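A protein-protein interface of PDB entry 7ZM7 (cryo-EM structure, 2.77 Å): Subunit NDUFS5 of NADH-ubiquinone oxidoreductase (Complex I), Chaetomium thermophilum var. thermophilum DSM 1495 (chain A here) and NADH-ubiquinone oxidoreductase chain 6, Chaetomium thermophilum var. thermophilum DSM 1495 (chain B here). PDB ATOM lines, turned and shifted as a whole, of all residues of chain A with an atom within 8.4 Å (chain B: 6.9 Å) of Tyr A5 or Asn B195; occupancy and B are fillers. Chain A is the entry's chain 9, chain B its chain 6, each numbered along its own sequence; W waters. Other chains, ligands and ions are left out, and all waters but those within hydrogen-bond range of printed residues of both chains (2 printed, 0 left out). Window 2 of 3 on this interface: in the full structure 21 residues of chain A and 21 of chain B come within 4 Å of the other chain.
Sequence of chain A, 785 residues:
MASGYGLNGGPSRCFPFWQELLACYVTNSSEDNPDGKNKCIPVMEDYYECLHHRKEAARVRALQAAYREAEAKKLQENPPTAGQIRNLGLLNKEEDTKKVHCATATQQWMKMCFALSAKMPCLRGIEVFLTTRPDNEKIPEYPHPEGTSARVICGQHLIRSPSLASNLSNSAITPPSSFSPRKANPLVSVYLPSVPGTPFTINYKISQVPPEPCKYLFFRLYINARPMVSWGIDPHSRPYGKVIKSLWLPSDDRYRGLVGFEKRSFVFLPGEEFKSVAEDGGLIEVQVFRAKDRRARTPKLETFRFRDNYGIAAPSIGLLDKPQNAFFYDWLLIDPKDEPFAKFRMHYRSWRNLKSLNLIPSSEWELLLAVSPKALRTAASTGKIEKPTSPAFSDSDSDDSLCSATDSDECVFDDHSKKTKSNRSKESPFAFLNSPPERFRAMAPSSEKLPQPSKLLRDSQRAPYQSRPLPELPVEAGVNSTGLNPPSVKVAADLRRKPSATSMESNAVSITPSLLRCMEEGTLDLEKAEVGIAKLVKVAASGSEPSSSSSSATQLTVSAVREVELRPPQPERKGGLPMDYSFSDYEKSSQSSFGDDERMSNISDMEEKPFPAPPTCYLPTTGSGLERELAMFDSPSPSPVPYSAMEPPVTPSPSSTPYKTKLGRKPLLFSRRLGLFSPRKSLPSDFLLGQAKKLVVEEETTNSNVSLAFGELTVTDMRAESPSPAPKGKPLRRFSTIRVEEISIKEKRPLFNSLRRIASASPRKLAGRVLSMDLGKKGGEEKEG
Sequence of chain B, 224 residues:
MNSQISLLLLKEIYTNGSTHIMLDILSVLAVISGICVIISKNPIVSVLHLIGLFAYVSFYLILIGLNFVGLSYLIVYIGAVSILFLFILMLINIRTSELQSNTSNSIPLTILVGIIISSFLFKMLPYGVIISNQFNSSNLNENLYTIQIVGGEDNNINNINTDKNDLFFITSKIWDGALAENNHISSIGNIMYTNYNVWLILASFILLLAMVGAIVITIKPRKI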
ATOM      1  N   ALA A   2      -6.636  20.259  -1.358  1.00  0.00           N
ATOM      2  CA  ALA A   2      -7.632  19.168  -1.526  1.00  0.00           C
ATOM      3  C   ALA A   2      -7.084  17.801  -1.093  1.00  0.00           C
ATOM      4  O   ALA A   2      -7.889  16.960  -0.703  1.00  0.00           O
ATOM      5  CB  ALA A   2      -8.225  19.151  -2.910  1.00  0.00           C
ATOM      6  N   SER A   3      -5.776  17.568  -1.212  1.00  0.00           N
ATOM      7  CA  SER A   3      -5.185  16.236  -0.902  1.00  0.00           C
ATOM      8  C   SER A   3      -5.354  15.834   0.569  1.00  0.00           C
ATOM      9  O   SER A   3      -5.675  14.664   0.799  1.00  0.00           O
ATOM     10  CB  SER A   3      -3.764  16.140  -1.332  1.00  0.00           C
ATOM     11  OG  SER A   3      -2.890  16.451  -0.264  1.00  0.00           O
ATOM     12  N   GLY A   4      -5.171  16.746   1.518  1.00  0.00           N
ATOM     13  CA  GLY A   4      -5.243  16.361   2.937  1.00  0.00           C
ATOM     14  C   GLY A   4      -3.874  16.269   3.567  1.00  0.00           C
ATOM     15  O   GLY A   4      -3.817  16.012   4.762  1.00  0.00           O
ATOM     16  N   TYR A   5      -2.810  16.408   2.780  1.00  0.00           N
ATOM     17  CA  TYR A   5      -1.424  16.268   3.283  1.00  0.00           C
ATOM     18  C   TYR A   5      -0.683  17.582   3.051  1.00  0.00           C
ATOM     19  O   TYR A   5      -0.600  18.034   1.906  1.00  0.00           O
ATOM     20  CB  TYR A   5      -0.782  15.004   2.704  1.00  0.00           C
ATOM     21  CG  TYR A   5      -1.641  13.775   2.845  1.00  0.00           C
ATOM     22  CD1 TYR A   5      -1.545  12.956   3.957  1.00  0.00           C
ATOM     23  CD2 TYR A   5      -2.579  13.454   1.881  1.00  0.00           C
ATOM     24  CE1 TYR A   5      -2.347  11.835   4.099  1.00  0.00           C
ATOM     25  CE2 TYR A   5      -3.394  12.343   2.010  1.00  0.00           C
ATOM     26  CZ  TYR A   5      -3.277  11.530   3.122  1.00  0.00           C
ATOM     27  OH  TYR A   5      -4.079  10.435   3.246  1.00  0.00           O
ATOM     28  N   GLY A   6      -0.130  18.168   4.106  1.00  0.00           N
ATOM     29  CA  GLY A   6       0.578  19.450   3.985  1.00  0.00           C
ATOM     30  C   GLY A   6       2.078  19.312   4.009  1.00  0.00           C
ATOM     31  O   GLY A   6       2.553  18.181   4.102  1.00  0.00           O
ATOM     32  N   LEU A   7       2.789  20.430   3.898  1.00  0.00           N
ATOM     33  CA  LEU A   7       4.271  20.437   3.845  1.00  0.00           C
ATOM     34  C   LEU A   7       4.934  19.974   5.146  1.00  0.00           C
ATOM     35  O   LEU A   7       6.019  19.400   5.047  1.00  0.00           O
ATOM     36  CB  LEU A   7       4.719  21.847   3.448  1.00  0.00           C
ATOM     37  CG  LEU A   7       4.027  22.438   2.219  1.00  0.00           C
ATOM     38  CD1 LEU A   7       4.549  23.833   1.925  1.00  0.00           C
ATOM     39  CD2 LEU A   7       4.202  21.540   1.008  1.00  0.00           C
ATOM     40  N   ASN A   8       4.322  20.208   6.305  1.00  0.00           N
ATOM     41  CA  ASN A   8       4.965  19.952   7.621  1.00  0.00           C
ATOM     42  C   ASN A   8       4.613  18.574   8.177  1.00  0.00           C
ATOM     43  O   ASN A   8       4.891  18.331   9.364  1.00  0.00           O
ATOM     44  CB  ASN A   8       4.563  21.021   8.636  1.00  0.00           C
ATOM     45  CG  ASN A   8       3.130  20.878   9.096  1.00  0.00           C
ATOM     46  OD1 ASN A   8       2.212  20.804   8.282  1.00  0.00           O
ATOM     47  ND2 ASN A   8       2.930  20.833  10.401  1.00  0.00           N
ATOM     48  N   GLY A   9       4.039  17.703   7.346  1.00  0.00           N
ATOM     49  CA  GLY A   9       3.624  16.363   7.803  1.00  0.00           C
ATOM     50  C   GLY A   9       2.179  16.356   8.259  1.00  0.00           C
ATOM     51  O   GLY A   9       1.609  15.265   8.365  1.00  0.00           O
ATOM     52  N   GLY A  10       1.616  17.530   8.548  1.00  0.00           N
ATOM     53  CA  GLY A  10       0.218  17.648   8.972  1.00  0.00           C
ATOM     54  C   GLY A  10      -0.719  17.797   7.792  1.00  0.00           C
ATOM     55  O   GLY A  10      -0.278  17.600   6.663  1.00  0.00           O
ATOM     56  N   PRO A  11      -2.014  18.077   8.022  1.00  0.00           N
ATOM     57  CA  PRO A  11      -2.999  18.203   6.950  1.00  0.00           C
ATOM     58  C   PRO A  11      -2.908  19.499   6.124  1.00  0.00           C
ATOM     59  O   PRO A  11      -2.220  20.399   6.544  1.00  0.00           O
ATOM     60  CB  PRO A  11      -4.327  18.105   7.708  1.00  0.00           C
ATOM     61  CG  PRO A  11      -3.971  17.627   9.096  1.00  0.00           C
ATOM     62  CD  PRO A  11      -2.611  18.226   9.344  1.00  0.00           C
ATOM     63  N   SER A  12      -3.551  19.538   4.950  1.00  0.00           N
ATOM     64  CA  SER A  12      -3.489  20.739   4.069  1.00  0.00           C
ATOM     65  C   SER A  12      -4.443  21.842   4.555  1.00  0.00           C
ATOM     66  O   SER A  12      -5.514  21.495   5.045  1.00  0.00           O
ATOM     67  CB  SER A  12      -3.644  20.400   2.605  1.00  0.00           C
ATOM     68  OG  SER A  12      -4.734  19.525   2.384  1.00  0.00           O
ATOM     69  N   ARG A  13      -4.085  23.118   4.387  1.00  0.00           N
ATOM     70  CA  ARG A  13      -4.867  24.269   4.928  1.00  0.00           C
ATOM     71  C   ARG A  13      -6.291  24.351   4.382  1.00  0.00           C
ATOM     72  O   ARG A  13      -7.173  24.740   5.153  1.00  0.00           O
ATOM     73  CB  ARG A  13      -4.104  25.583   4.732  1.00  0.00           C
ATOM     74  CG  ARG A  13      -3.738  25.903   3.293  1.00  0.00           C
ATOM     75  CD  ARG A  13      -2.987  27.216   3.231  1.00  0.00           C
ATOM     76  NE  ARG A  13      -2.901  27.655   1.852  1.00  0.00           N
ATOM     77  CZ  ARG A  13      -3.817  28.407   1.269  1.00  0.00           C
ATOM     78  NH1 ARG A  13      -3.682  28.755   0.003  1.00  0.00           N
ATOM     79  NH2 ARG A  13      -4.869  28.803   1.959  1.00  0.00           N
ATOM     80  N   PHE A  15      -8.076  21.872   3.082  1.00  0.00           N
ATOM     81  CA  PHE A  15      -8.778  20.564   3.067  1.00  0.00           C
ATOM     82  C   PHE A  15     -10.109  20.629   3.835  1.00  0.00           C
ATOM     83  O   PHE A  15     -11.048  19.968   3.379  1.00  0.00           O
ATOM     84  CB  PHE A  15      -7.806  19.468   3.500  1.00  0.00           C
ATOM     85  CG  PHE A  15      -8.348  18.064   3.501  1.00  0.00           C
ATOM     86  CD1 PHE A  15      -8.577  17.399   2.311  1.00  0.00           C
ATOM     87  CD2 PHE A  15      -8.588  17.395   4.687  1.00  0.00           C
ATOM     88  CE1 PHE A  15      -9.046  16.097   2.304  1.00  0.00           C
ATOM     89  CE2 PHE A  15      -9.060  16.094   4.678  1.00  0.00           C
ATOM     90  CZ  PHE A  15      -9.285  15.448   3.488  1.00  0.00           C
ATOM     91  N   SER B 187       7.592  14.147   4.720  1.00  0.00           N
ATOM     92  CA  SER B 187       6.163  14.281   4.356  1.00  0.00           C
ATOM     93  C   SER B 187       5.876  13.592   3.010  1.00  0.00           C
ATOM     94  O   SER B 187       4.845  12.923   2.927  1.00  0.00           O
ATOM     95  CB  SER B 187       5.782  15.720   4.380  1.00  0.00           C
ATOM     96  OG  SER B 187       6.350  16.360   5.506  1.00  0.00           O
ATOM     97  N   ASN B 190       5.996   9.822   3.734  1.00  0.00           N
ATOM     98  CA  ASN B 190       4.855   9.307   4.531  1.00  0.00           C
ATOM     99  C   ASN B 190       3.747   8.866   3.574  1.00  0.00           C
ATOM    100  O   ASN B 190       2.968   7.998   3.958  1.00  0.00           O
ATOM    101  CB  ASN B 190       4.309  10.339   5.520  1.00  0.00           C
ATOM    102  CG  ASN B 190       5.264  10.724   6.628  1.00  0.00           C
ATOM    103  OD1 ASN B 190       6.167   9.970   6.978  1.00  0.00           O
ATOM    104  ND2 ASN B 190       5.068  11.906   7.190  1.00  0.00           N
ATOM    105  N   ILE B 191       3.678   9.445   2.377  1.00  0.00           N
ATOM    106  CA  ILE B 191       2.560   9.118   1.448  1.00  0.00           C
ATOM    107  C   ILE B 191       3.068   8.508   0.128  1.00  0.00           C
ATOM    108  O   ILE B 191       2.260   7.853  -0.543  1.00  0.00           O
ATOM    109  CB  ILE B 191       1.680  10.371   1.240  1.00  0.00           C
ATOM    110  CG1 ILE B 191       2.420  11.459   0.463  1.00  0.00           C
ATOM    111  CG2 ILE B 191       1.137  10.889   2.560  1.00  0.00           C
ATOM    112  CD1 ILE B 191       1.513  12.361  -0.320  1.00  0.00           C
ATOM    113  N   MET B 192       4.343   8.688  -0.226  1.00  0.00           N
ATOM    114  CA  MET B 192       4.845   8.236  -1.519  1.00  0.00           C
ATOM    115  C   MET B 192       4.816   6.718  -1.659  1.00  0.00           C
ATOM    116  O   MET B 192       4.731   6.196  -2.776  1.00  0.00           O
ATOM    117  CB  MET B 192       6.257   8.781  -1.706  1.00  0.00           C
ATOM    118  CG  MET B 192       7.145   8.048  -2.657  1.00  0.00           C
ATOM    119  SD  MET B 192       8.715   8.864  -2.899  1.00  0.00           S
ATOM    120  CE  MET B 192       9.112   8.177  -4.492  1.00  0.00           C
ATOM    121  N   TYR B 193       4.899   5.990  -0.543  1.00  0.00           N
ATOM    122  CA  TYR B 193       5.018   4.512  -0.639  1.00  0.00           C
ATOM    123  C   TYR B 193       3.750   3.810  -0.160  1.00  0.00           C
ATOM    124  O   TYR B 193       3.721   2.587  -0.182  1.00  0.00           O
ATOM    125  CB  TYR B 193       6.242   4.029   0.142  1.00  0.00           C
ATOM    126  CG  TYR B 193       7.513   4.761  -0.183  1.00  0.00           C
ATOM    127  CD1 TYR B 193       8.345   4.333  -1.201  1.00  0.00           C
ATOM    128  CD2 TYR B 193       7.874   5.892   0.525  1.00  0.00           C
ATOM    129  CE1 TYR B 193       9.510   5.012  -1.509  1.00  0.00           C
ATOM    130  CE2 TYR B 193       9.027   6.588   0.226  1.00  0.00           C
ATOM    131  CZ  TYR B 193       9.849   6.142  -0.790  1.00  0.00           C
ATOM    132  OH  TYR B 193      10.993   6.823  -1.064  1.00  0.00           O
ATOM    133  N   THR B 194       2.734   4.557   0.260  1.00  0.00           N
ATOM    134  CA  THR B 194       1.509   3.926   0.831  1.00  0.00           C
ATOM    135  C   THR B 194       0.260   4.371   0.084  1.00  0.00           C
ATOM    136  O   THR B 194      -0.207   3.606  -0.740  1.00  0.00           O
ATOM    137  CB  THR B 194       1.407   4.221   2.332  1.00  0.00           C
ATOM    138  OG1 THR B 194       1.616   5.617   2.532  1.00  0.00           O
ATOM    139  CG2 THR B 194       2.405   3.439   3.156  1.00  0.00           C
ATOM    140  N   ASN B 195      -0.229   5.576   0.355  1.00  0.00           N
ATOM    141  CA  ASN B 195      -1.481   6.134  -0.217  1.00  0.00           C
ATOM    142  C   ASN B 195      -1.441   6.306  -1.732  1.00  0.00           C
ATOM    143  O   ASN B 195      -2.450   6.005  -2.370  1.00  0.00           O
ATOM    144  CB  ASN B 195      -1.721   7.514   0.389  1.00  0.00           C
ATOM    145  CG  ASN B 195      -2.001   7.532   1.875  1.00  0.00           C
ATOM    146  OD1 ASN B 195      -3.103   7.877   2.287  1.00  0.00           O
ATOM    147  ND2 ASN B 195      -1.012   7.201   2.685  1.00  0.00           N
ATOM    148  N   TYR B 196      -0.341   6.793  -2.280  1.00  0.00           N
ATOM    149  CA  TYR B 196      -0.245   7.067  -3.734  1.00  0.00           C
ATOM    150  C   TYR B 196       0.760   6.096  -4.356  1.00  0.00           C
ATOM    151  O   TYR B 196       1.423   6.489  -5.320  1.00  0.00           O
ATOM    152  CB  TYR B 196       0.043   8.549  -3.970  1.00  0.00           C
ATOM    153  CG  TYR B 196      -0.977   9.524  -3.440  1.00  0.00           C
ATOM    154  CD1 TYR B 196      -0.894  10.020  -2.150  1.00  0.00           C
ATOM    155  CD2 TYR B 196      -2.014   9.968  -4.237  1.00  0.00           C
ATOM    156  CE1 TYR B 196      -1.828  10.913  -1.658  1.00  0.00           C
ATOM    157  CE2 TYR B 196      -2.954  10.868  -3.766  1.00  0.00           C
ATOM    158  CZ  TYR B 196      -2.862  11.340  -2.471  1.00  0.00           C
ATOM    159  OH  TYR B 196      -3.788  12.224  -2.006  1.00  0.00           O
ATOM    160  N   ASN B 197       0.858   4.868  -3.834  1.00  0.00           N
ATOM    161  CA  ASN B 197       1.894   3.896  -4.289  1.00  0.00           C
ATOM    162  C   ASN B 197       1.679   3.414  -5.725  1.00  0.00           C
ATOM    163  O   ASN B 197       2.618   2.830  -6.273  1.00  0.00           O
ATOM    164  CB  ASN B 197       2.086   2.738  -3.303  1.00  0.00           C
ATOM    165  CG  ASN B 197       0.867   1.865  -3.098  1.00  0.00           C
ATOM    166  OD1 ASN B 197      -0.164   2.053  -3.738  1.00  0.00           O
ATOM    167  ND2 ASN B 197       0.978   0.901  -2.200  1.00  0.00           N
ATOM    168  N   VAL B 198       0.492   3.614  -6.295  1.00  0.00           N
ATOM    169  CA  VAL B 198       0.259   3.251  -7.727  1.00  0.00           C
ATOM    170  C   VAL B 198       1.155   4.132  -8.602  1.00  0.00           C
ATOM    171  O   VAL B 198       1.664   3.631  -9.618  1.00  0.00           O
ATOM    172  CB  VAL B 198      -1.238   3.308  -8.105  1.00  0.00           C
ATOM    173  CG1 VAL B 198      -1.488   3.801  -9.523  1.00  0.00           C
ATOM    174  CG2 VAL B 198      -1.913   1.967  -7.876  1.00  0.00           C
HETATM  175  O   HOH W   1      -4.428   9.515   0.452  1.00  0.00           O
HETATM  176  O   HOH W   2      -2.897   8.384   5.670  1.00  0.00           O
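The backbone carbonyl oxygen of Leu A7 lies within hydrogen-bond range of the side-chain hydroxyl of Ser B187, 3.1 Å away. OG of Ser B187 is in hydrogen-bond range of N of Gly A9, 3.2 Å away. OH of Tyr A5 is in hydrogen-bond range of OD1 of Asn B195 (2.9 Å).
O of Ile B191 lies within hydrogen-bond range of N of Tyr B196, at 3.3 Å. The side-chain hydroxyl (OG1) of Thr B194 lies within hydrogen-bond range of the side-chain amide nitrogen (ND2) of Asn B195 (3.1 Å). The side-chain hydroxyl (OG) of Ser A3 lies within hydrogen-bond range of the backbone NH (N) of Tyr A5 (3.0 Å). The backbone NH (N) of Gly A10 sits close to the side-chain amide oxygen (OD1) of Asn A8, 3.3 Å away.
Among the printed residues, pairs that only touch across the chains: Ser A3 with Tyr B196 (3.97 Å), Tyr A5 with Ile B191 (3.7 Å) and Asn A8 with Ser B187 (3.9 Å).
No residue of chain B comes within 4 Å of Gly A4. Tyr A5 touches two residues of chain B. Printed residues of chain B within 4 Å of Asn A8: Ser B187 (3.9 Å). Of the printed residues of chain A, Ser B187 touches Leu A7 (3.1 Å), Asn A8 (3.9 Å) and Gly A9 (3.2 Å). Printed residues of chain A within 4 Å of Ile B191: Tyr A5 (3.7 Å). Of chain A, only Tyr A5 comes within 4 Å of Asn B195. Of the printed residues of chain A, Tyr B196 touches Ser A3 (3.97 Å). The nearest residue of chain A that does not touch Asn B195 is Ser A3 (7.4 Å).
Hydrophobic or aromatic side chains of chain A that line the printed part of chain B: Tyr A5.
Water W1 lies within hydrogen-bond range of the side-chain amide oxygen of Asn B195 and the side-chain hydroxyl of Tyr A5. Water W2 bridges the side-chain hydroxyl (OH) of Tyr A5 and the side-chain amide oxygen (OD1) of Asn B195.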
